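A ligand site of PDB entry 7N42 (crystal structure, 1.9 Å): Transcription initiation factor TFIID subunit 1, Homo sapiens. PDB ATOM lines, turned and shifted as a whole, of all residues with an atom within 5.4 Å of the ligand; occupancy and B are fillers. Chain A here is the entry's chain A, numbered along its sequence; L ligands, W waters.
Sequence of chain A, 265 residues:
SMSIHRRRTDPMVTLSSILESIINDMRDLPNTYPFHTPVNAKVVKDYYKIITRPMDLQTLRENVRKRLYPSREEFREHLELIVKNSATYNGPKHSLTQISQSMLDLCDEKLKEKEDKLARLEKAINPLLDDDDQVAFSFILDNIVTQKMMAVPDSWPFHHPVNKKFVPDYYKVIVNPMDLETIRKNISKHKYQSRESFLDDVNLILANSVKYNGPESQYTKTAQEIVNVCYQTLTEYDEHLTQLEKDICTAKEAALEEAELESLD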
ATOM      1  N   TRP A 156     -21.931   1.418  15.297  1.00  0.00           N
ATOM      2  CA  TRP A 156     -21.216   1.355  14.026  1.00  0.00           C
ATOM      3  C   TRP A 156     -20.497   2.659  13.660  1.00  0.00           C
ATOM      4  O   TRP A 156     -19.418   2.578  13.042  1.00  0.00           O
ATOM      5  CB  TRP A 156     -22.185   0.935  12.891  1.00  0.00           C
ATOM      6  CG  TRP A 156     -23.280   1.937  12.625  1.00  0.00           C
ATOM      7  CD1 TRP A 156     -24.539   1.929  13.160  1.00  0.00           C
ATOM      8  CD2 TRP A 156     -23.208   3.101  11.782  1.00  0.00           C
ATOM      9  NE1 TRP A 156     -25.258   3.005  12.687  1.00  0.00           N
ATOM     10  CE2 TRP A 156     -24.462   3.747  11.856  1.00  0.00           C
ATOM     11  CE3 TRP A 156     -22.207   3.655  10.977  1.00  0.00           C
ATOM     12  CZ2 TRP A 156     -24.746   4.916  11.140  1.00  0.00           C
ATOM     13  CZ3 TRP A 156     -22.486   4.831  10.269  1.00  0.00           C
ATOM     14  CH2 TRP A 156     -23.753   5.447  10.361  1.00  0.00           C
ATOM     15  N   PRO A 157     -21.003   3.864  13.963  1.00  0.00           N
ATOM     16  CA  PRO A 157     -20.238   5.063  13.550  1.00  0.00           C
ATOM     17  C   PRO A 157     -18.852   5.148  14.155  1.00  0.00           C
ATOM     18  O   PRO A 157     -17.983   5.811  13.570  1.00  0.00           O
ATOM     19  CB  PRO A 157     -21.116   6.236  14.022  1.00  0.00           C
ATOM     20  CG  PRO A 157     -22.510   5.661  14.109  1.00  0.00           C
ATOM     21  CD  PRO A 157     -22.265   4.265  14.628  1.00  0.00           C
ATOM     22  N   PHE A 158     -18.605   4.445  15.256  1.00  0.00           N
ATOM     23  CA  PHE A 158     -17.370   4.521  16.034  1.00  0.00           C
ATOM     24  C   PHE A 158     -16.458   3.315  15.832  1.00  0.00           C
ATOM     25  O   PHE A 158     -15.371   3.293  16.417  1.00  0.00           O
ATOM     26  CB  PHE A 158     -17.705   4.616  17.534  1.00  0.00           C
ATOM     27  CG  PHE A 158     -18.649   5.732  17.876  1.00  0.00           C
ATOM     28  CD1 PHE A 158     -18.206   7.043  17.866  1.00  0.00           C
ATOM     29  CD2 PHE A 158     -19.998   5.491  18.046  1.00  0.00           C
ATOM     30  CE1 PHE A 158     -19.068   8.088  18.169  1.00  0.00           C
ATOM     31  CE2 PHE A 158     -20.883   6.543  18.313  1.00  0.00           C
ATOM     32  CZ  PHE A 158     -20.410   7.849  18.363  1.00  0.00           C
ATOM     33  N   HIS A 159     -16.827   2.372  14.964  1.00  0.00           N
ATOM     34  CA  HIS A 159     -16.036   1.155  14.749  1.00  0.00           C
ATOM     35  C   HIS A 159     -14.801   1.386  13.889  1.00  0.00           C
ATOM     36  O   HIS A 159     -13.876   0.573  13.936  1.00  0.00           O
ATOM     37  CB  HIS A 159     -16.919   0.082  14.097  1.00  0.00           C
ATOM     38  CG  HIS A 159     -17.941  -0.509  15.016  1.00  0.00           C
ATOM     39  ND1 HIS A 159     -18.468  -1.766  14.837  1.00  0.00           N
ATOM     40  CD2 HIS A 159     -18.438  -0.054  16.200  1.00  0.00           C
ATOM     41  CE1 HIS A 159     -19.322  -2.025  15.819  1.00  0.00           C
ATOM     42  NE2 HIS A 159     -19.311  -1.009  16.657  1.00  0.00           N
ATOM     43  N   HIS A 160     -14.796   2.411  13.046  1.00  0.00           N
ATOM     44  CA  HIS A 160     -13.736   2.624  12.065  1.00  0.00           C
ATOM     45  C   HIS A 160     -13.500   4.120  11.932  1.00  0.00           C
ATOM     46  O   HIS A 160     -14.376   4.925  12.309  1.00  0.00           O
ATOM     47  CB  HIS A 160     -14.089   2.007  10.716  1.00  0.00           C
ATOM     48  CG  HIS A 160     -14.358   0.543  10.796  1.00  0.00           C
ATOM     49  ND1 HIS A 160     -13.342  -0.389  10.870  1.00  0.00           N
ATOM     50  CD2 HIS A 160     -15.518  -0.163  10.858  1.00  0.00           C
ATOM     51  CE1 HIS A 160     -13.858  -1.597  10.943  1.00  0.00           C
ATOM     52  NE2 HIS A 160     -15.178  -1.491  10.938  1.00  0.00           N
ATOM     53  N   PRO A 161     -12.360   4.530  11.381  1.00  0.00           N
ATOM     54  CA  PRO A 161     -12.141   5.957  11.088  1.00  0.00           C
ATOM     55  C   PRO A 161     -13.185   6.496  10.127  1.00  0.00           C
ATOM     56  O   PRO A 161     -13.657   5.773   9.236  1.00  0.00           O
ATOM     57  CB  PRO A 161     -10.751   6.003  10.450  1.00  0.00           C
ATOM     58  CG  PRO A 161     -10.112   4.693  10.756  1.00  0.00           C
ATOM     59  CD  PRO A 161     -11.215   3.705  10.978  1.00  0.00           C
ATOM     60  N   VAL A 162     -13.603   7.743  10.360  1.00  0.00           N
ATOM     61  CA  VAL A 162     -14.514   8.407   9.433  1.00  0.00           C
ATOM     62  C   VAL A 162     -13.826   8.534   8.082  1.00  0.00           C
ATOM     63  O   VAL A 162     -12.665   8.956   7.996  1.00  0.00           O
ATOM     64  CB  VAL A 162     -14.941   9.776   9.994  1.00  0.00           C
ATOM     65  CG1 VAL A 162     -15.698  10.585   8.915  1.00  0.00           C
ATOM     66  CG2 VAL A 162     -15.727   9.608  11.248  1.00  0.00           C
ATOM     67  N   ASN A 163     -14.549   8.202   7.025  1.00  0.00           N
ATOM     68  CA  ASN A 163     -14.037   8.391   5.684  1.00  0.00           C
ATOM     69  C   ASN A 163     -14.460   9.785   5.218  1.00  0.00           C
ATOM     70  O   ASN A 163     -15.657  10.070   5.105  1.00  0.00           O
ATOM     71  CB  ASN A 163     -14.544   7.299   4.734  1.00  0.00           C
ATOM     72  CG  ASN A 163     -13.802   7.306   3.416  1.00  0.00           C
ATOM     73  OD1 ASN A 163     -13.392   8.349   2.914  1.00  0.00           O
ATOM     74  ND2 ASN A 163     -13.612   6.117   2.838  1.00  0.00           N
ATOM     75  N   PHE A 166     -17.295  10.546   2.797  1.00  0.00           N
ATOM     76  CA  PHE A 166     -18.691  10.520   3.205  1.00  0.00           C
ATOM     77  C   PHE A 166     -19.048  11.608   4.190  1.00  0.00           C
ATOM     78  O   PHE A 166     -20.218  12.014   4.243  1.00  0.00           O
ATOM     79  CB  PHE A 166     -18.999   9.175   3.860  1.00  0.00           C
ATOM     80  CG  PHE A 166     -18.719   8.009   2.971  1.00  0.00           C
ATOM     81  CD1 PHE A 166     -18.993   8.073   1.614  1.00  0.00           C
ATOM     82  CD2 PHE A 166     -18.114   6.867   3.477  1.00  0.00           C
ATOM     83  CE1 PHE A 166     -18.713   7.002   0.786  1.00  0.00           C
ATOM     84  CE2 PHE A 166     -17.824   5.795   2.658  1.00  0.00           C
ATOM     85  CZ  PHE A 166     -18.124   5.867   1.308  1.00  0.00           C
ATOM     86  N   VAL A 167     -18.089  12.129   4.942  1.00  0.00           N
ATOM     87  CA  VAL A 167     -18.318  13.222   5.882  1.00  0.00           C
ATOM     88  C   VAL A 167     -17.255  14.281   5.619  1.00  0.00           C
ATOM     89  O   VAL A 167     -16.225  14.330   6.317  1.00  0.00           O
ATOM     90  CB  VAL A 167     -18.285  12.714   7.341  1.00  0.00           C
ATOM     91  CG1 VAL A 167     -18.804  13.776   8.291  1.00  0.00           C
ATOM     92  CG2 VAL A 167     -19.080  11.414   7.485  1.00  0.00           C
ATOM     93  N   TYR A 170     -15.437  16.452   8.407  1.00  0.00           N
ATOM     94  CA  TYR A 170     -15.212  15.848   9.718  1.00  0.00           C
ATOM     95  C   TYR A 170     -13.866  16.241  10.318  1.00  0.00           C
ATOM     96  O   TYR A 170     -13.786  16.587  11.504  1.00  0.00           O
ATOM     97  CB  TYR A 170     -15.296  14.329   9.633  1.00  0.00           C
ATOM     98  CG  TYR A 170     -15.188  13.695  11.004  1.00  0.00           C
ATOM     99  CD1 TYR A 170     -16.245  13.723  11.901  1.00  0.00           C
ATOM    100  CD2 TYR A 170     -13.985  13.112  11.432  1.00  0.00           C
ATOM    101  CE1 TYR A 170     -16.143  13.158  13.158  1.00  0.00           C
ATOM    102  CE2 TYR A 170     -13.864  12.545  12.709  1.00  0.00           C
ATOM    103  CZ  TYR A 170     -14.946  12.584  13.553  1.00  0.00           C
ATOM    104  OH  TYR A 170     -14.841  12.025  14.817  1.00  0.00           O
ATOM    105  N   MET A 178     -10.305   9.655  16.710  1.00  0.00           N
ATOM    106  CA  MET A 178     -10.132   8.338  17.327  1.00  0.00           C
ATOM    107  C   MET A 178     -11.334   7.453  17.024  1.00  0.00           C
ATOM    108  O   MET A 178     -12.443   7.944  16.841  1.00  0.00           O
ATOM    109  CB  MET A 178      -9.948   8.454  18.860  1.00  0.00           C
ATOM    110  CG  MET A 178      -9.498   7.146  19.566  1.00  0.00           C
ATOM    111  SD  MET A 178      -8.090   6.293  18.846  1.00  0.00           S
ATOM    112  CE  MET A 178      -6.819   7.583  18.873  1.00  0.00           C
ATOM    113  N   ASP A 179     -11.091   6.138  16.973  1.00  0.00           N
ATOM    114  CA  ASP A 179     -12.154   5.189  16.666  1.00  0.00           C
ATOM    115  C   ASP A 179     -11.752   3.854  17.277  1.00  0.00           C
ATOM    116  O   ASP A 179     -10.596   3.655  17.666  1.00  0.00           O
ATOM    117  CB  ASP A 179     -12.342   5.065  15.156  1.00  0.00           C
ATOM    118  CG  ASP A 179     -11.122   4.515  14.515  1.00  0.00           C
ATOM    119  OD1 ASP A 179     -10.232   5.324  14.162  1.00  0.00           O
ATOM    120  OD2 ASP A 179     -11.059   3.276  14.350  1.00  0.00           O
ATOM    121  N   LEU A 180     -12.692   2.905  17.306  1.00  0.00           N
ATOM    122  CA  LEU A 180     -12.416   1.648  17.988  1.00  0.00           C
ATOM    123  C   LEU A 180     -11.430   0.770  17.229  1.00  0.00           C
ATOM    124  O   LEU A 180     -10.697  -0.006  17.862  1.00  0.00           O
ATOM    125  CB  LEU A 180     -13.722   0.895  18.255  1.00  0.00           C
ATOM    126  CG  LEU A 180     -14.653   1.654  19.204  1.00  0.00           C
ATOM    127  CD1 LEU A 180     -15.999   0.923  19.315  1.00  0.00           C
ATOM    128  CD2 LEU A 180     -13.999   1.884  20.572  1.00  0.00           C
ATOM    129  N   ILE A 205     -12.892   9.529  22.008  1.00  0.00           N
ATOM    130  CA  ILE A 205     -14.051   9.260  21.143  1.00  0.00           C
ATOM    131  C   ILE A 205     -15.283  10.052  21.607  1.00  0.00           C
ATOM    132  O   ILE A 205     -15.991  10.679  20.805  1.00  0.00           O
ATOM    133  CB  ILE A 205     -14.354   7.757  21.074  1.00  0.00           C
ATOM    134  CG1 ILE A 205     -13.163   7.010  20.478  1.00  0.00           C
ATOM    135  CG2 ILE A 205     -15.646   7.509  20.261  1.00  0.00           C
ATOM    136  CD1 ILE A 205     -13.321   5.488  20.434  1.00  0.00           C
ATOM    137  N   SER A 209     -17.227  13.262  19.803  1.00  0.00           N
ATOM    138  CA  SER A 209     -18.653  13.263  19.444  1.00  0.00           C
ATOM    139  C   SER A 209     -19.358  14.489  20.021  1.00  0.00           C
ATOM    140  O   SER A 209     -20.205  15.084  19.350  1.00  0.00           O
ATOM    141  CB  SER A 209     -19.358  11.981  19.898  1.00  0.00           C
ATOM    142  OG  SER A 209     -20.701  11.990  19.431  1.00  0.00           O
ATOM    143  N   TYR A 212     -18.338  17.350  17.601  1.00  0.00           N
ATOM    144  CA  TYR A 212     -18.829  17.321  16.227  1.00  0.00           C
ATOM    145  C   TYR A 212     -20.346  17.228  16.143  1.00  0.00           C
ATOM    146  O   TYR A 212     -20.965  17.925  15.333  1.00  0.00           O
ATOM    147  CB  TYR A 212     -18.159  16.160  15.455  1.00  0.00           C
ATOM    148  CG  TYR A 212     -18.532  16.206  13.995  1.00  0.00           C
ATOM    149  CD1 TYR A 212     -17.903  17.080  13.124  1.00  0.00           C
ATOM    150  CD2 TYR A 212     -19.505  15.349  13.474  1.00  0.00           C
ATOM    151  CE1 TYR A 212     -18.267  17.150  11.795  1.00  0.00           C
ATOM    152  CE2 TYR A 212     -19.872  15.413  12.138  1.00  0.00           C
ATOM    153  CZ  TYR A 212     -19.248  16.312  11.304  1.00  0.00           C
ATOM    154  OH  TYR A 212     -19.602  16.381   9.986  1.00  0.00           O
ATOM    155  N   ASN A 213     -20.962  16.427  17.001  1.00  0.00           N
ATOM    156  CA  ASN A 213     -22.393  16.166  16.933  1.00  0.00           C
ATOM    157  C   ASN A 213     -23.219  16.952  17.930  1.00  0.00           C
ATOM    158  O   ASN A 213     -24.404  17.187  17.682  1.00  0.00           O
ATOM    159  CB  ASN A 213     -22.666  14.676  17.152  1.00  0.00           C
ATOM    160  CG  ASN A 213     -21.973  13.808  16.125  1.00  0.00           C
ATOM    161  OD1 ASN A 213     -22.142  14.001  14.929  1.00  0.00           O
ATOM    162  ND2 ASN A 213     -21.147  12.878  16.599  1.00  0.00           N
ATOM    163  N   TYR A 219     -25.597  10.245  18.355  1.00  0.00           N
ATOM    164  CA  TYR A 219     -24.218   9.781  18.270  1.00  0.00           C
ATOM    165  C   TYR A 219     -23.509   9.895  19.612  1.00  0.00           C
ATOM    166  O   TYR A 219     -22.784   8.978  20.028  1.00  0.00           O
ATOM    167  CB  TYR A 219     -23.422  10.621  17.254  1.00  0.00           C
ATOM    168  CG  TYR A 219     -23.768  10.417  15.798  1.00  0.00           C
ATOM    169  CD1 TYR A 219     -23.384   9.257  15.134  1.00  0.00           C
ATOM    170  CD2 TYR A 219     -24.465  11.383  15.094  1.00  0.00           C
ATOM    171  CE1 TYR A 219     -23.698   9.062  13.797  1.00  0.00           C
ATOM    172  CE2 TYR A 219     -24.777  11.208  13.767  1.00  0.00           C
ATOM    173  CZ  TYR A 219     -24.397  10.051  13.117  1.00  0.00           C
ATOM    174  OH  TYR A 219     -24.715   9.883  11.786  1.00  0.00           O
HETATM  175  C1  LIG L   1     -21.458   7.534   6.007  1.00  0.00           C
HETATM  176  N1  LIG L   1     -23.524   8.437   5.257  1.00  0.00           N
HETATM  177  C2  LIG L   1     -23.875   8.804   6.526  1.00  0.00           C
HETATM  178  C3  LIG L   1     -23.671   9.041   8.745  1.00  0.00           C
HETATM  179  C4  LIG L   1     -18.061   5.167   8.991  1.00  0.00           C
HETATM  180  C5  LIG L   1     -17.950   3.731   9.517  1.00  0.00           C
HETATM  181  C6  LIG L   1     -18.991   8.648  12.811  1.00  0.00           C
HETATM  182  C7  LIG L   1     -19.647  10.730  14.101  1.00  0.00           C
HETATM  183  C8  LIG L   1     -20.560  11.184  12.915  1.00  0.00           C
HETATM  184  C9  LIG L   1     -20.642  10.401  11.768  1.00  0.00           C
HETATM  185  C10 LIG L   1     -19.860   9.099  11.690  1.00  0.00           C
HETATM  186  C11 LIG L   1     -19.878   8.171  10.464  1.00  0.00           C
HETATM  187  C12 LIG L   1     -20.777   7.591   8.444  1.00  0.00           C
HETATM  188  C13 LIG L   1     -21.795   7.880   7.330  1.00  0.00           C
HETATM  189  C14 LIG L   1     -22.378   7.821   4.985  1.00  0.00           C
HETATM  190  C15 LIG L   1     -23.024   8.540   7.578  1.00  0.00           C
HETATM  191  C16 LIG L   1     -24.887   9.583   8.345  1.00  0.00           C
HETATM  192  C17 LIG L   1     -19.005   6.355   9.213  1.00  0.00           C
HETATM  193  C18 LIG L   1     -18.343   4.453   6.616  1.00  0.00           C
HETATM  194  C19 LIG L   1     -17.132   4.859  10.170  1.00  0.00           C
HETATM  195  C20 LIG L   1     -18.927   7.141  10.373  1.00  0.00           C
HETATM  196  C21 LIG L   1     -18.049   9.019  15.091  1.00  0.00           C
HETATM  197  C22 LIG L   1     -16.579   8.996  14.615  1.00  0.00           C
HETATM  198  C23 LIG L   1     -15.676   8.187  15.573  1.00  0.00           C
HETATM  199  C24 LIG L   1     -15.093   7.087  15.109  1.00  0.00           C
HETATM  200  C25 LIG L   1     -21.505  11.051  10.871  1.00  0.00           C
HETATM  201  C26 LIG L   1     -21.928  12.215  11.494  1.00  0.00           C
HETATM  202  N2  LIG L   1     -20.760   8.379   9.506  1.00  0.00           N
HETATM  203  N3  LIG L   1     -24.993   9.429   7.019  1.00  0.00           N
HETATM  204  N4  LIG L   1     -19.916   6.594   8.285  1.00  0.00           N
HETATM  205  N5  LIG L   1     -15.801   4.637   7.535  1.00  0.00           N
HETATM  206  N6  LIG L   1     -18.915   9.456  13.996  1.00  0.00           N
HETATM  207  N7  LIG L   1     -21.351  12.284  12.732  1.00  0.00           N
HETATM  208  O1  LIG L   1     -19.536  11.390  15.097  1.00  0.00           O
HETATM  209  O2  LIG L   1     -16.882   6.856   7.041  1.00  0.00           O
HETATM  210  S1  LIG L   1     -17.090   5.463   7.455  1.00  0.00           S
HETATM  211  O   HOH W   1     -16.175  10.307  18.078  1.00  0.00           O
HETATM  212  O   HOH W   2     -24.822   9.610   3.045  1.00  0.00           O
HETATM  213  O   HOH W   3     -17.245  12.279  16.420  1.00  0.00           O
HETATM  214  O   HOH W   4     -18.609   0.864  10.975  1.00  0.00           O
HETATM  215  O   HOH W   5     -26.326  11.429   5.648  1.00  0.00           O
HETATM  216  O   HOH W   6     -15.433   1.710   7.224  1.00  0.00           O
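A nitrogen (N5) of the ligand sits at hydrogen-bond distance from the backbone carbonyl oxygen (O) of Pro 161 (3.0 Å).
N of Asn 163 is in hydrogen-bond range of O2 of the ligand (2.7 Å).
O1 of the ligand is in hydrogen-bond range of ND2 of Asn 213, 2.7 Å away.
The side-chain amide nitrogen (ND2) of Asn 213 lies within hydrogen-bond range of the side-chain hydroxyl (OG) of Ser 209 (3.0 Å).
The backbone NH (N) of Leu 180 is in hydrogen-bond range of the backbone carbonyl oxygen (O) of Phe 158 (2.8 Å).
Trp 156 touches the ligand.
Pro 157 touches the ligand.
CE1 of Phe 158 touches C21 of the ligand (3.4 Å).
His 160 touches the ligand (O to C19, 3.5 Å).
CG2 of Val 162 touches C22 of the ligand, at 3.5 Å.
Phe 166 touches the ligand (CB to C1, 3.7 Å).
Tyr 170 touches the ligand.
Met 178 touches the ligand.
CB of Asp 179 touches C24 of the ligand, 3.4 Å away.
Tyr 212 touches the ligand.
Tyr 219 touches the ligand (OH to C3, 3.3 Å).
Hydrophobic or aromatic side chains within 4 Å of the ligand: Trp 156, Pro 157, Phe 158, Val 162, Phe 166, Tyr 212 and Tyr 219.
Within 4 Å of the ligand: Trp 156, Pro 157, Phe 158, His 160, Pro 161, Val 162, Asn 163, Phe 166, Tyr 170, Met 178, Asp 179, Tyr 212, Asn 213 and Tyr 219.
Water W3 lies within hydrogen-bond range of an oxygen (O1) of the ligand (2.8 Å) and the side-chain hydroxyl (OH) of Tyr 170 (2.9 Å).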
